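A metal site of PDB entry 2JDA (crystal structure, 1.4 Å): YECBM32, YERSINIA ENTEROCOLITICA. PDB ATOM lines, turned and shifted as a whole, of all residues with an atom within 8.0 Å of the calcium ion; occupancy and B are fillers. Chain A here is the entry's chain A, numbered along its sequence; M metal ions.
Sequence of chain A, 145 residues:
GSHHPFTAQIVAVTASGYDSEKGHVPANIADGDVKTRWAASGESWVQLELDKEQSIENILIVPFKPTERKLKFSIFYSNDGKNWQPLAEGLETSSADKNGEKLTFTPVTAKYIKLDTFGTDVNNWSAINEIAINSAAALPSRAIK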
ATOM      1  N   VAL A  25       3.570 -22.344  13.402  1.00  0.00           N
ATOM      2  CA  VAL A  25       2.929 -22.700  14.652  1.00  0.00           C
ATOM      3  C   VAL A  25       2.445 -21.450  15.407  1.00  0.00           C
ATOM      4  O   VAL A  25       2.976 -20.366  15.198  1.00  0.00           O
ATOM      5  CB  VAL A  25       3.885 -23.518  15.568  1.00  0.00           C
ATOM      6  CG1 VAL A  25       4.163 -24.912  14.969  1.00  0.00           C
ATOM      7  CG2 VAL A  25       5.178 -22.739  15.862  1.00  0.00           C
ATOM      8  N   PRO A  26       1.485 -21.630  16.300  1.00  0.00           N
ATOM      9  CA  PRO A  26       0.970 -20.485  17.059  1.00  0.00           C
ATOM     10  C   PRO A  26       2.038 -19.677  17.826  1.00  0.00           C
ATOM     11  O   PRO A  26       2.031 -18.439  17.808  1.00  0.00           O
ATOM     12  CB  PRO A  26      -0.053 -21.146  17.984  1.00  0.00           C
ATOM     13  CG  PRO A  26      -0.534 -22.310  17.200  1.00  0.00           C
ATOM     14  CD  PRO A  26       0.726 -22.860  16.580  1.00  0.00           C
ATOM     15  N   ALA A  27       3.023 -20.344  18.431  1.00  0.00           N
ATOM     16  CA  ALA A  27       4.037 -19.631  19.183  1.00  0.00           C
ATOM     17  C   ALA A  27       4.841 -18.651  18.346  1.00  0.00           C
ATOM     18  O   ALA A  27       5.471 -17.727  18.840  1.00  0.00           O
ATOM     19  CB  ALA A  27       4.909 -20.595  19.918  1.00  0.00           C
ATOM     20  N   ASN A  28       4.883 -18.881  17.034  1.00  0.00           N
ATOM     21  CA  ASN A  28       5.582 -17.990  16.123  1.00  0.00           C
ATOM     22  C   ASN A  28       4.990 -16.586  16.142  1.00  0.00           C
ATOM     23  O   ASN A  28       5.603 -15.657  15.630  1.00  0.00           O
ATOM     24  CB  ASN A  28       5.582 -18.481  14.662  1.00  0.00           C
ATOM     25  CG  ASN A  28       6.535 -19.634  14.335  1.00  0.00           C
ATOM     26  OD1 ASN A  28       6.466 -20.190  13.189  1.00  0.00           O
ATOM     27  ND2 ASN A  28       7.363 -19.974  15.235  1.00  0.00           N
ATOM     28  N   ILE A  29       3.768 -16.420  16.636  1.00  0.00           N
ATOM     29  CA  ILE A  29       3.147 -15.105  16.607  1.00  0.00           C
ATOM     30  C   ILE A  29       3.715 -14.205  17.687  1.00  0.00           C
ATOM     31  O   ILE A  29       3.442 -13.016  17.660  1.00  0.00           O
ATOM     32  CB  ILE A  29       1.584 -15.264  16.773  1.00  0.00           C
ATOM     33  CG1 ILE A  29       0.871 -14.124  16.099  1.00  0.00           C
ATOM     34  CG2 ILE A  29       1.172 -15.393  18.232  1.00  0.00           C
ATOM     35  CD1 ILE A  29      -0.644 -14.256  16.129  1.00  0.00           C
ATOM     36  N   ALA A  30       4.458 -14.771  18.647  1.00  0.00           N
ATOM     37  CA  ALA A  30       4.895 -14.029  19.825  1.00  0.00           C
ATOM     38  C   ALA A  30       6.347 -14.269  20.181  1.00  0.00           C
ATOM     39  O   ALA A  30       6.704 -14.145  21.373  1.00  0.00           O
ATOM     40  CB  ALA A  30       3.995 -14.381  20.989  1.00  0.00           C
ATOM     41  N   ASP A  31       7.172 -14.603  19.182  1.00  0.00           N
ATOM     42  CA  ASP A  31       8.577 -14.980  19.430  1.00  0.00           C
ATOM     43  C   ASP A  31       9.546 -13.861  19.204  1.00  0.00           C
ATOM     44  O   ASP A  31      10.763 -14.064  19.343  1.00  0.00           O
ATOM     45  CB  ASP A  31       8.978 -16.213  18.618  1.00  0.00           C
ATOM     46  CG  ASP A  31       8.858 -16.038  17.147  1.00  0.00           C
ATOM     47  OD1 ASP A  31       8.455 -14.942  16.662  1.00  0.00           O
ATOM     48  OD2 ASP A  31       9.247 -16.924  16.380  1.00  0.00           O
ATOM     49  N   GLY A  32       9.038 -12.685  18.884  1.00  0.00           N
ATOM     50  CA  GLY A  32       9.897 -11.532  18.673  1.00  0.00           C
ATOM     51  C   GLY A  32      10.631 -11.528  17.366  1.00  0.00           C
ATOM     52  O   GLY A  32      11.485 -10.653  17.103  1.00  0.00           O
ATOM     53  N   ASP A  33      10.257 -12.412  16.463  1.00  0.00           N
ATOM     54  CA  ASP A  33      10.900 -12.549  15.184  1.00  0.00           C
ATOM     55  C   ASP A  33       9.864 -12.328  14.045  1.00  0.00           C
ATOM     56  O   ASP A  33       8.986 -13.171  13.857  1.00  0.00           O
ATOM     57  CB  ASP A  33      11.505 -13.957  15.131  1.00  0.00           C
ATOM     58  CG  ASP A  33      12.340 -14.203  13.900  1.00  0.00           C
ATOM     59  OD1 ASP A  33      12.288 -13.394  12.950  1.00  0.00           O
ATOM     60  OD2 ASP A  33      13.092 -15.197  13.819  1.00  0.00           O
ATOM     61  N   VAL A  34       9.949 -11.225  13.319  1.00  0.00           N
ATOM     62  CA  VAL A  34       8.985 -10.974  12.256  1.00  0.00           C
ATOM     63  C   VAL A  34       9.129 -11.937  11.081  1.00  0.00           C
ATOM     64  O   VAL A  34       8.262 -11.941  10.213  1.00  0.00           O
ATOM     65  CB  VAL A  34       9.038  -9.528  11.735  1.00  0.00           C
ATOM     66  CG1 VAL A  34       8.625  -8.603  12.858  1.00  0.00           C
ATOM     67  CG2 VAL A  34      10.406  -9.217  11.136  1.00  0.00           C
ATOM     68  N   LYS A  35      10.220 -12.720  11.007  1.00  0.00           N
ATOM     69  CA  LYS A  35      10.377 -13.682   9.939  1.00  0.00           C
ATOM     70  C   LYS A  35       9.631 -15.012  10.196  1.00  0.00           C
ATOM     71  O   LYS A  35       9.582 -15.843   9.319  1.00  0.00           O
ATOM     72  CB  LYS A  35      11.851 -14.035   9.690  1.00  0.00           C
ATOM     73  CG  LYS A  35      12.742 -12.848   9.414  1.00  0.00           C
ATOM     74  CD  LYS A  35      14.251 -13.321   9.549  1.00  0.00           C
ATOM     75  CE  LYS A  35      14.789 -13.434  11.035  1.00  0.00           C
ATOM     76  NZ  LYS A  35      14.480 -12.303  11.984  1.00  0.00           N
ATOM     77  N   THR A  36       9.171 -15.258  11.421  1.00  0.00           N
ATOM     78  CA  THR A  36       8.357 -16.470  11.683  1.00  0.00           C
ATOM     79  C   THR A  36       6.896 -16.018  11.831  1.00  0.00           C
ATOM     80  O   THR A  36       6.608 -14.932  12.348  1.00  0.00           O
ATOM     81  CB  THR A  36       8.760 -17.138  12.991  1.00  0.00           C
ATOM     82  OG1 THR A  36       8.483 -16.250  14.085  1.00  0.00           O
ATOM     83  CG2 THR A  36      10.234 -17.459  13.006  1.00  0.00           C
ATOM     84  N   ARG A  37       5.978 -16.867  11.411  1.00  0.00           N
ATOM     85  CA  ARG A  37       4.544 -16.563  11.456  1.00  0.00           C
ATOM     86  C   ARG A  37       3.730 -17.744  11.896  1.00  0.00           C
ATOM     87  O   ARG A  37       4.129 -18.872  11.770  1.00  0.00           O
ATOM     88  CB  ARG A  37       4.072 -16.087  10.099  1.00  0.00           C
ATOM     89  CG  ARG A  37       4.130 -17.084   8.963  1.00  0.00           C
ATOM     90  CD  ARG A  37       3.765 -16.467   7.646  1.00  0.00           C
ATOM     91  NE  ARG A  37       3.868 -17.342   6.474  1.00  0.00           N
ATOM     92  CZ  ARG A  37       4.962 -17.510   5.781  1.00  0.00           C
ATOM     93  NH1 ARG A  37       6.123 -16.982   6.160  1.00  0.00           N
ATOM     94  NH2 ARG A  37       4.884 -18.272   4.705  1.00  0.00           N
ATOM     95  N   TRP A  38       2.583 -17.412  12.466  1.00  0.00           N
ATOM     96  CA  TRP A  38       1.452 -18.323  12.588  1.00  0.00           C
ATOM     97  C   TRP A  38       0.611 -18.162  11.338  1.00  0.00           C
ATOM     98  O   TRP A  38       0.335 -17.042  10.903  1.00  0.00           O
ATOM     99  CB  TRP A  38       0.601 -17.947  13.807  1.00  0.00           C
ATOM    100  CG  TRP A  38      -0.718 -18.658  13.857  1.00  0.00           C
ATOM    101  CD1 TRP A  38      -0.905 -20.012  14.041  1.00  0.00           C
ATOM    102  CD2 TRP A  38      -2.021 -18.103  13.706  1.00  0.00           C
ATOM    103  NE1 TRP A  38      -2.236 -20.337  13.934  1.00  0.00           N
ATOM    104  CE2 TRP A  38      -2.948 -19.170  13.793  1.00  0.00           C
ATOM    105  CE3 TRP A  38      -2.510 -16.802  13.474  1.00  0.00           C
ATOM    106  CZ2 TRP A  38      -4.313 -18.967  13.645  1.00  0.00           C
ATOM    107  CZ3 TRP A  38      -3.851 -16.608  13.344  1.00  0.00           C
ATOM    108  CH2 TRP A  38      -4.754 -17.703  13.441  1.00  0.00           C
ATOM    109  N   VAL A  62       1.413  -7.313  13.186  1.00  0.00           N
ATOM    110  CA  VAL A  62       2.325  -7.335  12.050  1.00  0.00           C
ATOM    111  C   VAL A  62       1.857  -8.485  11.131  1.00  0.00           C
ATOM    112  O   VAL A  62       2.327  -9.609  11.240  1.00  0.00           O
ATOM    113  CB  VAL A  62       3.772  -7.494  12.509  1.00  0.00           C
ATOM    114  CG1 VAL A  62       4.727  -7.374  11.297  1.00  0.00           C
ATOM    115  CG2 VAL A  62       4.135  -6.488  13.632  1.00  0.00           C
ATOM    116  N   ILE A 128       0.044 -14.176  10.470  1.00  0.00           N
ATOM    117  CA  ILE A 128       0.489 -13.069  11.317  1.00  0.00           C
ATOM    118  C   ILE A 128       1.925 -13.319  11.734  1.00  0.00           C
ATOM    119  O   ILE A 128       2.221 -14.332  12.335  1.00  0.00           O
ATOM    120  CB  ILE A 128      -0.447 -12.857  12.543  1.00  0.00           C
ATOM    121  CG1 ILE A 128      -1.878 -12.569  12.074  1.00  0.00           C
ATOM    122  CG2 ILE A 128       0.083 -11.748  13.371  1.00  0.00           C
ATOM    123  CD1 ILE A 128      -2.964 -12.587  13.191  1.00  0.00           C
ATOM    124  N   ASN A 129       2.805 -12.368  11.413  1.00  0.00           N
ATOM    125  CA  ASN A 129       4.202 -12.497  11.790  1.00  0.00           C
ATOM    126  C   ASN A 129       4.427 -12.281  13.274  1.00  0.00           C
ATOM    127  O   ASN A 129       5.223 -12.980  13.930  1.00  0.00           O
ATOM    128  CB  ASN A 129       5.080 -11.513  11.016  1.00  0.00           C
ATOM    129  CG  ASN A 129       5.063 -11.710   9.507  1.00  0.00           C
ATOM    130  OD1 ASN A 129       4.795 -12.793   8.994  1.00  0.00           O
ATOM    131  ND2 ASN A 129       5.367 -10.608   8.752  1.00  0.00           N
ATOM    132  N   GLU A 130       3.756 -11.279  13.843  1.00  0.00           N
ATOM    133  CA  GLU A 130       3.992 -10.919  15.225  1.00  0.00           C
ATOM    134  C   GLU A 130       2.792 -10.115  15.751  1.00  0.00           C
ATOM    135  O   GLU A 130       2.086  -9.395  15.040  1.00  0.00           O
ATOM    136  CB  GLU A 130       5.254 -10.052  15.304  1.00  0.00           C
ATOM    137  CG  GLU A 130       5.948 -10.103  16.615  1.00  0.00           C
ATOM    138  CD  GLU A 130       6.610 -11.424  17.007  1.00  0.00           C
ATOM    139  OE1 GLU A 130       6.974 -12.368  16.221  1.00  0.00           O
ATOM    140  OE2 GLU A 130       6.670 -11.530  18.189  1.00  0.00           O
ATOM    141  N   ILE A 131       2.527 -10.362  17.032  1.00  0.00           N
ATOM    142  CA  ILE A 131       1.611  -9.591  17.815  1.00  0.00           C
ATOM    143  C   ILE A 131       2.272  -9.261  19.128  1.00  0.00           C
ATOM    144  O   ILE A 131       2.944 -10.088  19.740  1.00  0.00           O
ATOM    145  CB  ILE A 131       0.310 -10.358  18.017  1.00  0.00           C
ATOM    146  CG1 ILE A 131      -0.809  -9.489  18.531  1.00  0.00           C
ATOM    147  CG2 ILE A 131       0.519 -11.512  18.859  1.00  0.00           C
ATOM    148  CD1 ILE A 131      -2.151  -9.934  17.873  1.00  0.00           C
HETATM  149 CA    CA M   1       7.110 -14.239  14.667  1.00  0.00          CA
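The calcium ion is bound by O of Asn 28 (2.3 Å), O of Asp 33 (2.3 Å), O of Asn 129 (2.4 Å), OE1 of Glu 130 (2.4 Å), O of Thr 36 (2.5 Å), OG1 of Thr 36 (2.5 Å) and OD1 of Asp 31 (2.5 Å). The calcium ion has seven donor atoms within binding distance.
Six residues have an atom within 4 Å of the calcium ion: Asn 28, Asp 31, Asp 33, Thr 36, Asn 129 and Glu 130. The nearest printed residue that does not touch the calcium ion is Arg 37 (4.3 Å).
O of Arg 37 sits close to OD1 of Asn 28 (3.0 Å). The side-chain carboxylate (OD1) of Asp 33 lies within salt-bridge range of the side-chain amino group (NZ) of Lys 35 (2.6 Å). The backbone NH of Asn 129 is in hydrogen-bond range of the backbone carbonyl oxygen of Val 62 (2.8 Å). The side-chain carboxylate of Glu 130 is in hydrogen-bond range of the backbone NH of Gly 32 (2.7 Å). N of Val 62 sits at hydrogen-bond distance from O of Glu 130, at 2.9 Å.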
